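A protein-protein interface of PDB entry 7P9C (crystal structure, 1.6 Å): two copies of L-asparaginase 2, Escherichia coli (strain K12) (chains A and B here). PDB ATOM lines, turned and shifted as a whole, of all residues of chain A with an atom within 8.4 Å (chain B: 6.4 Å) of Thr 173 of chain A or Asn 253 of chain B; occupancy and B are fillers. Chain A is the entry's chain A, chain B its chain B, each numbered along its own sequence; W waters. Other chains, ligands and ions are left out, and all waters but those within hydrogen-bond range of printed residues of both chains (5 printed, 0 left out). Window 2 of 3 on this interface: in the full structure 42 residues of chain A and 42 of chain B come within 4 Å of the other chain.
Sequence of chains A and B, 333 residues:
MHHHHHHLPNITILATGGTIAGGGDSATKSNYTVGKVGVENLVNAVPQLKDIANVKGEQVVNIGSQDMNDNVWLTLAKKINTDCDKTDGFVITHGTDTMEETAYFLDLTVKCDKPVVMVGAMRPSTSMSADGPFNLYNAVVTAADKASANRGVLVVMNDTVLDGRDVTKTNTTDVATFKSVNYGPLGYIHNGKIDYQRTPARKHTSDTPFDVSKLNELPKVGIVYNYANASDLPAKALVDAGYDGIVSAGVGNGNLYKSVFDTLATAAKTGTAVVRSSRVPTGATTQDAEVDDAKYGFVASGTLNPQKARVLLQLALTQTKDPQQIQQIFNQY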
ATOM      1  N   GLN A  66     -19.865   8.781 -22.931  1.00  0.00           N
ATOM      2  CA  GLN A  66     -20.744   9.073 -24.058  1.00  0.00           C
ATOM      3  C   GLN A  66     -20.278   8.393 -25.338  1.00  0.00           C
ATOM      4  O   GLN A  66     -21.060   8.301 -26.305  1.00  0.00           O
ATOM      5  CB  GLN A  66     -20.860  10.586 -24.291  1.00  0.00           C
ATOM      6  CG  GLN A  66     -19.669  11.215 -25.001  1.00  0.00           C
ATOM      7  CD  GLN A  66     -18.485  11.503 -24.107  1.00  0.00           C
ATOM      8  OE1 GLN A  66     -18.472  11.186 -22.916  1.00  0.00           O
ATOM      9  NE2 GLN A  66     -17.447  12.081 -24.703  1.00  0.00           N
ATOM     10  N   THR A  96     -20.865   8.490 -15.936  1.00  0.00           N
ATOM     11  CA  THR A  96     -22.273   8.326 -15.600  1.00  0.00           C
ATOM     12  C   THR A  96     -23.217   8.280 -16.802  1.00  0.00           C
ATOM     13  O   THR A  96     -24.284   7.669 -16.681  1.00  0.00           O
ATOM     14  CB  THR A  96     -22.723   9.435 -14.637  1.00  0.00           C
ATOM     15  OG1 THR A  96     -22.535  10.732 -15.236  1.00  0.00           O
ATOM     16  CG2 THR A  96     -21.911   9.326 -13.346  1.00  0.00           C
ATOM     17  N   ASP A  97     -22.843   8.855 -17.954  1.00  0.00           N
ATOM     18  CA  ASP A  97     -23.798   9.018 -19.054  1.00  0.00           C
ATOM     19  C   ASP A  97     -24.369   7.680 -19.548  1.00  0.00           C
ATOM     20  O   ASP A  97     -25.550   7.610 -19.883  1.00  0.00           O
ATOM     21  CB  ASP A  97     -23.147   9.756 -20.220  1.00  0.00           C
ATOM     22  CG  ASP A  97     -22.914  11.218 -19.930  1.00  0.00           C
ATOM     23  OD1 ASP A  97     -23.243  11.687 -18.814  1.00  0.00           O
ATOM     24  OD2 ASP A  97     -22.348  11.921 -20.814  1.00  0.00           O
ATOM     25  N   ALA A 121     -19.026   9.357 -10.762  1.00  0.00           N
ATOM     26  CA  ALA A 121     -19.108  10.617 -10.027  1.00  0.00           C
ATOM     27  C   ALA A 121     -19.826  11.654 -10.881  1.00  0.00           C
ATOM     28  O   ALA A 121     -19.510  11.792 -12.062  1.00  0.00           O
ATOM     29  CB  ALA A 121     -17.705  11.125  -9.664  1.00  0.00           C
ATOM     30  N   MET A 122     -20.759  12.398 -10.274  1.00  0.00           N
ATOM     31  CA  MET A 122     -21.493  13.470 -10.947  1.00  0.00           C
ATOM     32  C   MET A 122     -20.817  14.824 -10.859  1.00  0.00           C
ATOM     33  O   MET A 122     -21.215  15.734 -11.592  1.00  0.00           O
ATOM     34  CB  MET A 122     -22.932  13.566 -10.389  1.00  0.00           C
ATOM     35  CG  MET A 122     -23.703  12.333 -10.767  1.00  0.00           C
ATOM     36  SD  MET A 122     -24.072  12.357 -12.557  1.00  0.00           S
ATOM     37  CE  MET A 122     -25.132  13.773 -12.733  1.00  0.00           C
ATOM     38  N   ARG A 123     -19.788  14.973 -10.027  1.00  0.00           N
ATOM     39  CA  ARG A 123     -18.978  16.181  -9.929  1.00  0.00           C
ATOM     40  C   ARG A 123     -17.533  15.850 -10.260  1.00  0.00           C
ATOM     41  O   ARG A 123     -17.064  14.750  -9.949  1.00  0.00           O
ATOM     42  CB  ARG A 123     -19.055  16.784  -8.521  1.00  0.00           C
ATOM     43  CG  ARG A 123     -20.458  17.220  -8.148  1.00  0.00           C
ATOM     44  CD  ARG A 123     -20.542  17.819  -6.756  1.00  0.00           C
ATOM     45  NE  ARG A 123     -21.880  18.295  -6.438  1.00  0.00           N
ATOM     46  CZ  ARG A 123     -22.351  18.407  -5.209  1.00  0.00           C
ATOM     47  NH1 ARG A 123     -21.605  18.107  -4.157  1.00  0.00           N
ATOM     48  NH2 ARG A 123     -23.594  18.841  -5.029  1.00  0.00           N
ATOM     49  N   ASP A 131     -18.030  14.072  -5.245  1.00  0.00           N
ATOM     50  CA  ASP A 131     -18.690  12.870  -4.738  1.00  0.00           C
ATOM     51  C   ASP A 131     -17.905  11.582  -5.003  1.00  0.00           C
ATOM     52  O   ASP A 131     -18.162  10.549  -4.360  1.00  0.00           O
ATOM     53  CB  ASP A 131     -20.109  12.744  -5.330  1.00  0.00           C
ATOM     54  CG  ASP A 131     -20.170  12.833  -6.894  1.00  0.00           C
ATOM     55  OD1 ASP A 131     -19.347  13.540  -7.524  1.00  0.00           O
ATOM     56  OD2 ASP A 131     -21.066  12.143  -7.475  1.00  0.00           O
ATOM     57  N   LYS A 169     -30.200   6.754 -14.923  1.00  0.00           N
ATOM     58  CA  LYS A 169     -29.885   8.151 -14.624  1.00  0.00           C
ATOM     59  C   LYS A 169     -31.151   8.992 -14.744  1.00  0.00           C
ATOM     60  O   LYS A 169     -31.690   9.135 -15.836  1.00  0.00           O
ATOM     61  CB  LYS A 169     -28.796   8.626 -15.590  1.00  0.00           C
ATOM     62  CG  LYS A 169     -28.096   9.868 -15.170  1.00  0.00           C
ATOM     63  CD  LYS A 169     -26.912  10.205 -16.088  1.00  0.00           C
ATOM     64  CE  LYS A 169     -26.293  11.545 -15.766  1.00  0.00           C
ATOM     65  NZ  LYS A 169     -24.859  11.683 -16.191  1.00  0.00           N
ATOM     66  N   THR A 170     -31.631   9.570 -13.642  1.00  0.00           N
ATOM     67  CA  THR A 170     -32.907  10.271 -13.677  1.00  0.00           C
ATOM     68  C   THR A 170     -32.784  11.789 -13.787  1.00  0.00           C
ATOM     69  O   THR A 170     -33.777  12.448 -14.111  1.00  0.00           O
ATOM     70  CB  THR A 170     -33.753   9.970 -12.432  1.00  0.00           C
ATOM     71  OG1 THR A 170     -33.149  10.555 -11.275  1.00  0.00           O
ATOM     72  CG2 THR A 170     -33.925   8.470 -12.191  1.00  0.00           C
ATOM     73  N   ASN A 171     -31.608  12.360 -13.512  1.00  0.00           N
ATOM     74  CA  ASN A 171     -31.387  13.807 -13.547  1.00  0.00           C
ATOM     75  C   ASN A 171     -30.049  14.117 -14.196  1.00  0.00           C
ATOM     76  O   ASN A 171     -29.067  13.394 -14.005  1.00  0.00           O
ATOM     77  CB  ASN A 171     -31.440  14.366 -12.133  1.00  0.00           C
ATOM     78  CG  ASN A 171     -31.391  15.865 -12.088  1.00  0.00           C
ATOM     79  OD1 ASN A 171     -30.308  16.463 -11.978  1.00  0.00           O
ATOM     80  ND2 ASN A 171     -32.567  16.492 -12.157  1.00  0.00           N
ATOM     81  N   THR A 172     -29.990  15.235 -14.923  1.00  0.00           N
ATOM     82  CA  THR A 172     -28.799  15.532 -15.694  1.00  0.00           C
ATOM     83  C   THR A 172     -27.608  15.942 -14.838  1.00  0.00           C
ATOM     84  O   THR A 172     -26.487  15.862 -15.341  1.00  0.00           O
ATOM     85  CB  THR A 172     -29.078  16.653 -16.691  1.00  0.00           C
ATOM     86  OG1 THR A 172     -29.656  17.760 -15.977  1.00  0.00           O
ATOM     87  CG2 THR A 172     -30.067  16.233 -17.780  1.00  0.00           C
ATOM     88  N   THR A 173     -27.812  16.430 -13.601  1.00  0.00           N
ATOM     89  CA  THR A 173     -26.710  16.958 -12.792  1.00  0.00           C
ATOM     90  C   THR A 173     -26.673  16.505 -11.334  1.00  0.00           C
ATOM     91  O   THR A 173     -25.612  16.633 -10.715  1.00  0.00           O
ATOM     92  CB  THR A 173     -26.716  18.497 -12.811  1.00  0.00           C
ATOM     93  OG1 THR A 173     -27.933  19.002 -12.245  1.00  0.00           O
ATOM     94  CG2 THR A 173     -26.611  19.024 -14.229  1.00  0.00           C
ATOM     95  N   ASP A 174     -27.760  15.995 -10.756  1.00  0.00           N
ATOM     96  CA  ASP A 174     -27.845  15.737  -9.316  1.00  0.00           C
ATOM     97  C   ASP A 174     -26.951  14.575  -8.919  1.00  0.00           C
ATOM     98  O   ASP A 174     -26.945  13.531  -9.573  1.00  0.00           O
ATOM     99  CB  ASP A 174     -29.329  15.499  -9.008  1.00  0.00           C
ATOM    100  CG  ASP A 174     -29.681  15.261  -7.531  1.00  0.00           C
ATOM    101  OD1 ASP A 174     -28.864  15.174  -6.606  1.00  0.00           O
ATOM    102  OD2 ASP A 174     -30.923  15.280  -7.281  1.00  0.00           O
ATOM    103  N   VAL A 175     -26.219  14.745  -7.816  1.00  0.00           N
ATOM    104  CA  VAL A 175     -25.421  13.640  -7.288  1.00  0.00           C
ATOM    105  C   VAL A 175     -26.280  12.434  -6.933  1.00  0.00           C
ATOM    106  O   VAL A 175     -25.769  11.307  -6.920  1.00  0.00           O
ATOM    107  CB  VAL A 175     -24.595  14.071  -6.062  1.00  0.00           C
ATOM    108  CG1 VAL A 175     -23.580  15.125  -6.450  1.00  0.00           C
ATOM    109  CG2 VAL A 175     -25.494  14.543  -4.964  1.00  0.00           C
ATOM    110  N   ALA A 176     -27.585  12.635  -6.692  1.00  0.00           N
ATOM    111  CA  ALA A 176     -28.515  11.564  -6.358  1.00  0.00           C
ATOM    112  C   ALA A 176     -29.263  11.000  -7.576  1.00  0.00           C
ATOM    113  O   ALA A 176     -30.289  10.339  -7.419  1.00  0.00           O
ATOM    114  CB  ALA A 176     -29.524  12.059  -5.325  1.00  0.00           C
ATOM    115  N   THR A 177     -28.737  11.211  -8.766  1.00  0.00           N
ATOM    116  CA  THR A 177     -29.445  10.907 -10.001  1.00  0.00           C
ATOM    117  C   THR A 177     -29.770   9.430 -10.205  1.00  0.00           C
ATOM    118  O   THR A 177     -30.806   9.122 -10.807  1.00  0.00           O
ATOM    119  CB  THR A 177     -28.597  11.431 -11.160  1.00  0.00           C
ATOM    120  OG1 THR A 177     -29.284  11.222 -12.382  1.00  0.00           O
ATOM    121  CG2 THR A 177     -27.236  10.759 -11.236  1.00  0.00           C
ATOM    122  N   GLY B 250     -29.614  13.574 -25.999  1.00  0.00           N
ATOM    123  CA  GLY B 250     -28.271  13.214 -25.598  1.00  0.00           C
ATOM    124  C   GLY B 250     -28.224  12.376 -24.331  1.00  0.00           C
ATOM    125  O   GLY B 250     -29.232  12.115 -23.669  1.00  0.00           O
ATOM    126  N   VAL B 251     -27.026  11.954 -23.997  1.00  0.00           N
ATOM    127  CA  VAL B 251     -26.799  11.213 -22.759  1.00  0.00           C
ATOM    128  C   VAL B 251     -26.314  12.183 -21.679  1.00  0.00           C
ATOM    129  O   VAL B 251     -25.609  13.159 -21.968  1.00  0.00           O
ATOM    130  CB  VAL B 251     -25.817  10.039 -22.974  1.00  0.00           C
ATOM    131  CG1 VAL B 251     -26.457   8.985 -23.908  1.00  0.00           C
ATOM    132  CG2 VAL B 251     -24.477  10.464 -23.542  1.00  0.00           C
ATOM    133  N   GLY B 252     -26.694  11.924 -20.432  1.00  0.00           N
ATOM    134  CA  GLY B 252     -26.329  12.842 -19.375  1.00  0.00           C
ATOM    135  C   GLY B 252     -26.737  14.271 -19.686  1.00  0.00           C
ATOM    136  O   GLY B 252     -27.849  14.543 -20.145  1.00  0.00           O
ATOM    137  N   ASN B 253     -25.822  15.205 -19.415  1.00  0.00           N
ATOM    138  CA  ASN B 253     -26.055  16.632 -19.645  1.00  0.00           C
ATOM    139  C   ASN B 253     -25.858  16.985 -21.120  1.00  0.00           C
ATOM    140  O   ASN B 253     -24.972  17.747 -21.512  1.00  0.00           O
ATOM    141  CB  ASN B 253     -25.117  17.438 -18.765  1.00  0.00           C
ATOM    142  CG  ASN B 253     -25.509  18.903 -18.645  1.00  0.00           C
ATOM    143  OD1 ASN B 253     -26.366  19.423 -19.370  1.00  0.00           O
ATOM    144  ND2 ASN B 253     -24.826  19.585 -17.752  1.00  0.00           N
ATOM    145  N   GLY B 254     -26.706  16.382 -21.942  1.00  0.00           N
ATOM    146  CA  GLY B 254     -26.753  16.685 -23.352  1.00  0.00           C
ATOM    147  C   GLY B 254     -25.578  16.225 -24.186  1.00  0.00           C
ATOM    148  O   GLY B 254     -25.339  16.776 -25.269  1.00  0.00           O
ATOM    149  N   ASN B 255     -24.859  15.207 -23.748  1.00  0.00           N
ATOM    150  CA  ASN B 255     -23.709  14.755 -24.521  1.00  0.00           C
ATOM    151  C   ASN B 255     -24.118  13.845 -25.679  1.00  0.00           C
ATOM    152  O   ASN B 255     -25.221  13.289 -25.724  1.00  0.00           O
ATOM    153  CB  ASN B 255     -22.725  14.036 -23.612  1.00  0.00           C
ATOM    154  CG  ASN B 255     -22.059  15.001 -22.627  1.00  0.00           C
ATOM    155  OD1 ASN B 255     -21.577  16.071 -23.016  1.00  0.00           O
ATOM    156  ND2 ASN B 255     -22.054  14.640 -21.355  1.00  0.00           N
ATOM    157  N   ARG B 276     -29.173  20.607 -28.412  1.00  0.00           N
ATOM    158  CA  ARG B 276     -28.845  19.536 -27.474  1.00  0.00           C
ATOM    159  C   ARG B 276     -29.880  19.500 -26.357  1.00  0.00           C
ATOM    160  O   ARG B 276     -29.968  20.439 -25.558  1.00  0.00           O
ATOM    161  CB  ARG B 276     -27.460  19.741 -26.878  1.00  0.00           C
ATOM    162  CG  ARG B 276     -26.345  19.799 -27.911  1.00  0.00           C
ATOM    163  CD  ARG B 276     -24.966  19.748 -27.204  1.00  0.00           C
ATOM    164  NE  ARG B 276     -24.776  20.864 -26.290  1.00  0.00           N
ATOM    165  CZ  ARG B 276     -24.802  20.770 -24.968  1.00  0.00           C
ATOM    166  NH1 ARG B 276     -24.977  19.608 -24.360  1.00  0.00           N
ATOM    167  NH2 ARG B 276     -24.679  21.880 -24.241  1.00  0.00           N
ATOM    168  N   SER B 277     -30.629  18.390 -26.275  1.00  0.00           N
ATOM    169  CA  SER B 277     -31.470  18.048 -25.143  1.00  0.00           C
ATOM    170  C   SER B 277     -30.886  16.776 -24.514  1.00  0.00           C
ATOM    171  O   SER B 277     -29.734  16.390 -24.798  1.00  0.00           O
ATOM    172  CB  SER B 277     -32.923  17.879 -25.617  1.00  0.00           C
ATOM    173  OG  SER B 277     -33.846  17.584 -24.569  1.00  0.00           O
ATOM    174  N   SER B 278     -31.690  16.090 -23.711  1.00  0.00           N
ATOM    175  CA  SER B 278     -31.225  14.893 -23.034  1.00  0.00           C
ATOM    176  C   SER B 278     -32.341  13.857 -22.965  1.00  0.00           C
ATOM    177  O   SER B 278     -33.507  14.199 -22.752  1.00  0.00           O
ATOM    178  CB  SER B 278     -30.752  15.200 -21.621  1.00  0.00           C
ATOM    179  OG  SER B 278     -30.284  14.031 -20.998  1.00  0.00           O
ATOM    180  N   VAL B 280     -32.350  12.008 -20.490  1.00  0.00           N
ATOM    181  CA  VAL B 280     -32.523  11.898 -19.040  1.00  0.00           C
ATOM    182  C   VAL B 280     -33.791  12.638 -18.651  1.00  0.00           C
ATOM    183  O   VAL B 280     -34.015  13.760 -19.126  1.00  0.00           O
ATOM    184  CB  VAL B 280     -31.305  12.468 -18.326  1.00  0.00           C
ATOM    185  CG1 VAL B 280     -31.482  12.461 -16.811  1.00  0.00           C
ATOM    186  CG2 VAL B 280     -30.045  11.680 -18.704  1.00  0.00           C
ATOM    187  N   THR B 282     -35.285  14.237 -16.084  1.00  0.00           N
ATOM    188  CA  THR B 282     -35.371  15.490 -15.357  1.00  0.00           C
ATOM    189  C   THR B 282     -34.034  16.206 -15.423  1.00  0.00           C
ATOM    190  O   THR B 282     -32.998  15.595 -15.691  1.00  0.00           O
ATOM    191  CB  THR B 282     -35.779  15.282 -13.887  1.00  0.00           C
ATOM    192  OG1 THR B 282     -34.695  14.701 -13.145  1.00  0.00           O
ATOM    193  CG2 THR B 282     -36.991  14.361 -13.759  1.00  0.00           C
ATOM    194  N   GLY B 283     -34.030  17.507 -15.101  1.00  0.00           N
ATOM    195  CA  GLY B 283     -32.811  18.287 -15.090  1.00  0.00           C
ATOM    196  C   GLY B 283     -32.689  19.117 -16.332  1.00  0.00           C
ATOM    197  O   GLY B 283     -33.574  19.037 -17.182  1.00  0.00           O
ATOM    198  N   ALA B 284     -31.623  19.910 -16.432  1.00  0.00           N
ATOM    199  CA  ALA B 284     -31.428  20.803 -17.569  1.00  0.00           C
ATOM    200  C   ALA B 284     -30.204  20.473 -18.367  1.00  0.00           C
ATOM    201  O   ALA B 284     -29.184  20.114 -17.783  1.00  0.00           O
ATOM    202  CB  ALA B 284     -31.332  22.244 -17.095  1.00  0.00           C
ATOM    203  N   THR B 285     -30.310  20.545 -19.691  1.00  0.00           N
ATOM    204  CA  THR B 285     -29.153  20.389 -20.539  1.00  0.00           C
ATOM    205  C   THR B 285     -28.660  21.848 -20.464  1.00  0.00           C
ATOM    206  O   THR B 285     -29.293  22.711 -21.001  1.00  0.00           O
ATOM    207  CB  THR B 285     -29.470  19.886 -21.940  1.00  0.00           C
ATOM    208  OG1 THR B 285     -29.879  18.532 -21.839  1.00  0.00           O
ATOM    209  CG2 THR B 285     -28.254  20.005 -22.846  1.00  0.00           C
ATOM    210  N   THR B 286     -27.520  22.053 -19.832  1.00  0.00           N
ATOM    211  CA  THR B 286     -27.034  23.385 -19.534  1.00  0.00           C
ATOM    212  C   THR B 286     -26.054  23.901 -20.584  1.00  0.00           C
ATOM    213  O   THR B 286     -25.374  23.143 -21.281  1.00  0.00           O
ATOM    214  CB  THR B 286     -26.351  23.405 -18.153  1.00  0.00           C
ATOM    215  OG1 THR B 286     -25.177  22.561 -18.164  1.00  0.00           O
ATOM    216  CG2 THR B 286     -27.276  22.896 -17.076  1.00  0.00           C
ATOM    217  N   GLN B 287     -25.944  25.209 -20.617  1.00  0.00           N
ATOM    218  CA  GLN B 287     -24.874  25.780 -21.364  1.00  0.00           C
ATOM    219  C   GLN B 287     -23.665  25.677 -20.374  1.00  0.00           C
ATOM    220  O   GLN B 287     -23.856  25.332 -19.217  1.00  0.00           O
ATOM    221  CB  GLN B 287     -25.160  27.243 -21.715  1.00  0.00           C
ATOM    222  CG  GLN B 287     -26.371  27.491 -22.596  1.00  0.00           C
ATOM    223  CD  GLN B 287     -26.707  28.967 -22.706  1.00  0.00           C
ATOM    224  OE1 GLN B 287     -27.588  29.467 -22.015  1.00  0.00           O
ATOM    225  NE2 GLN B 287     -25.991  29.668 -23.559  1.00  0.00           N
ATOM    226  N   ALA B 289     -21.162  23.492 -20.038  1.00  0.00           N
ATOM    227  CA  ALA B 289     -20.859  22.157 -19.536  1.00  0.00           C
ATOM    228  C   ALA B 289     -19.777  21.515 -20.395  1.00  0.00           C
ATOM    229  O   ALA B 289     -18.755  22.149 -20.657  1.00  0.00           O
ATOM    230  CB  ALA B 289     -22.124  21.296 -19.509  1.00  0.00           C
ATOM    231  N   GLU B 290     -19.977  20.280 -20.858  1.00  0.00           N
ATOM    232  CA  GLU B 290     -18.919  19.585 -21.589  1.00  0.00           C
ATOM    233  C   GLU B 290     -18.931  19.849 -23.091  1.00  0.00           C
ATOM    234  O   GLU B 290     -18.019  19.382 -23.784  1.00  0.00           O
ATOM    235  CB  GLU B 290     -18.997  18.073 -21.346  1.00  0.00           C
ATOM    236  CG  GLU B 290     -18.039  17.573 -20.266  1.00  0.00           C
ATOM    237  CD  GLU B 290     -17.824  16.060 -20.296  1.00  0.00           C
ATOM    238  OE1 GLU B 290     -18.269  15.399 -21.263  1.00  0.00           O
ATOM    239  OE2 GLU B 290     -17.198  15.533 -19.344  1.00  0.00           O
ATOM    240  N   VAL B 291     -19.900  20.601 -23.615  1.00  0.00           N
ATOM    241  CA  VAL B 291     -19.943  20.925 -25.043  1.00  0.00           C
ATOM    242  C   VAL B 291     -19.827  22.434 -25.210  1.00  0.00           C
ATOM    243  O   VAL B 291     -20.594  23.183 -24.594  1.00  0.00           O
ATOM    244  CB  VAL B 291     -21.228  20.407 -25.719  1.00  0.00           C
ATOM    245  CG1 VAL B 291     -21.264  20.821 -27.168  1.00  0.00           C
ATOM    246  CG2 VAL B 291     -21.323  18.887 -25.608  1.00  0.00           C
HETATM  247  O   HOH W   1     -23.219  14.446 -18.365  1.00  0.00           O
HETATM  248  O   HOH W   2     -19.776  12.182 -20.712  1.00  0.00           O
HETATM  249  O   HOH W   3     -29.871  19.465 -13.735  1.00  0.00           O
HETATM  250  O   HOH W   4     -34.887  18.707 -11.961  1.00  0.00           O
HETATM  251  O   HOH W   5     -27.616   9.374 -19.642  1.00  0.00           O
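OD2 of Asp 97 of chain A sits at hydrogen-bond distance from ND2 of Asn 255 of chain B (2.8 Å).
OG1 of Thr 282 of chain B sits at hydrogen-bond distance from O of Thr 170 of chain A, 2.6 Å away.
The side-chain amide nitrogen (ND2) of Asn 171 of chain A is in hydrogen-bond range of the side-chain hydroxyl (OG1) of Thr 282 of chain B (3.0 Å).
The side-chain amide nitrogen (ND2) of Asn 171 of chain A sits close to the backbone NH (N) of Gly 283 of chain B (3.4 Å).
N of Thr 172 of chain A sits at hydrogen-bond distance from O of Thr 282 of chain B.
OG1 of Thr 172 of chain A lies within hydrogen-bond range of N of Ala 284 of chain B, at 2.9 Å.
Of the 16 printed residues of chain A, 7 touch a printed residue of chain B.
Hydrophobic or aromatic side chains of chain B within 4 Å of the printed part of chain A: Val 251 and Val 280.
Among the printed residues, 19 pairs touch across the chains.
Printed residues of chain B within 4 Å of Asn 171 of chain A: Val 280 (3.3 Å), Thr 282 (3.0 Å) and Gly 283 (3.4 Å).
Of the printed residues of chain B, Thr 172 of chain A touches Gly 252, Ser 278, Val 280, Thr 282, Gly 283 and Ala 284.
Of the printed residues of chain B, Thr 173 of chain A touches Asn 253 (3.99 Å).
Gly 252 of chain B touches three residues of chain A.
Of the printed residues of chain A, Asn 253 of chain B touches Thr 173.
No residue of chain A comes within 4 Å of Gly 254 of chain B.
Of the printed residues of chain A, Ser 278 of chain B touches Thr 172 (3.9 Å).
Of the printed residues of chain A, Val 280 of chain B touches Lys 169 (3.5 Å), Thr 170 (3.4 Å), Asn 171 (3.3 Å) and Thr 172 (3.7 Å).
Printed residues of chain A within 4 Å of Ala 284 of chain B: Thr 172.
Thr 285 of chain B touches none of the printed residues of chain A.
The nearest printed residue of chain A that does not touch Asn 253 of chain B is Thr 172 of chain A (4.01 Å).
The nearest printed residue of chain B that does not touch Thr 172 of chain A is Asn 253 of chain B (4.01 Å).
No position is printed for both chains.
Of the 19 pairs that touch across the chains among the printed residues, none has its exchanged pair printed and touching as well.
Water W3 lies within hydrogen-bond range of the side-chain hydroxyl (OG1) of Thr 173 of chain A, the side-chain hydroxyl (OG1) of Thr 172 of chain A and the backbone NH (N) of Ala 284 of chain B.
Water W2 lies within hydrogen-bond range of OD2 of Asp 97 of chain A (2.6 Å), OE1 of Gln 66 of chain A (2.7 Å) and ND2 of Asn 255 of chain B (3.4 Å).
Water W5 lies within hydrogen-bond range of the backbone carbonyl oxygen of Asp 97 of chain A (2.7 Å) and the backbone NH of Gly 252 of chain B (2.8 Å).
Water W1 lies within hydrogen-bond range of the side-chain carboxylate of Asp 97 of chain A (2.8 Å), the backbone NH of Asn 253 of chain B (2.9 Å) and the side-chain amide nitrogen of Asn 255 of chain B (3.2 Å).
Water W4 bridges ND2 of Asn 171 of chain A (3.2 Å) and N of Gly 283 of chain B (3.5 Å).
Among the printed residues, merely in contact across the chains: Asn 171 of chain A with Val 280 of chain B (3.3 Å), Thr 172 of chain A with Gly 283 of chain B (3.3 Å), Asp 97 of chain A with Gly 252 of chain B (3.3 Å), Thr 170 of chain A with Val 280 of chain B (3.4 Å), Lys 169 of chain A with Val 280 of chain B (3.5 Å), Asp 97 of chain A with Val 251 of chain B (3.6 Å), Thr 172 of chain A with Gly 252 of chain B (3.7 Å), Thr 172 of chain A with Val 280 of chain B (3.7 Å), Lys 169 of chain A with Gly 252 of chain B (3.7 Å), Gln 66 of chain A with Val 251 of chain B (3.7 Å), Thr 172 of chain A with Ser 278 of chain B (3.9 Å), Gln 66 of chain A with Asn 255 of chain B (3.98 Å) and Thr 173 of chain A with Asn 253 of chain B (3.99 Å).
OD1 of Asp 97 of chain A lies within salt-bridge range of NZ of Lys 169 of chain A, 3.1 Å away.
The side-chain amide oxygen (OD1) of Asn 171 of chain A is in hydrogen-bond range of the backbone NH (N) of Asp 174 of chain A, at 2.9 Å.
The side-chain hydroxyl (OG1) of Thr 177 of chain A sits at hydrogen-bond distance from the backbone carbonyl oxygen (O) of Asn 171 of chain A, at 2.7 Å.
O of Gly 252 of chain B lies within hydrogen-bond range of OG of Ser 278 of chain B, 2.6 Å away.
The side-chain amide oxygen (OD1) of Asn 253 of chain B sits close to the backbone carbonyl oxygen (O) of Ala 284 of chain B (3.3 Å).
N of Thr 286 of chain B is in hydrogen-bond range of OD1 of Asn 253 of chain B (2.9 Å).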
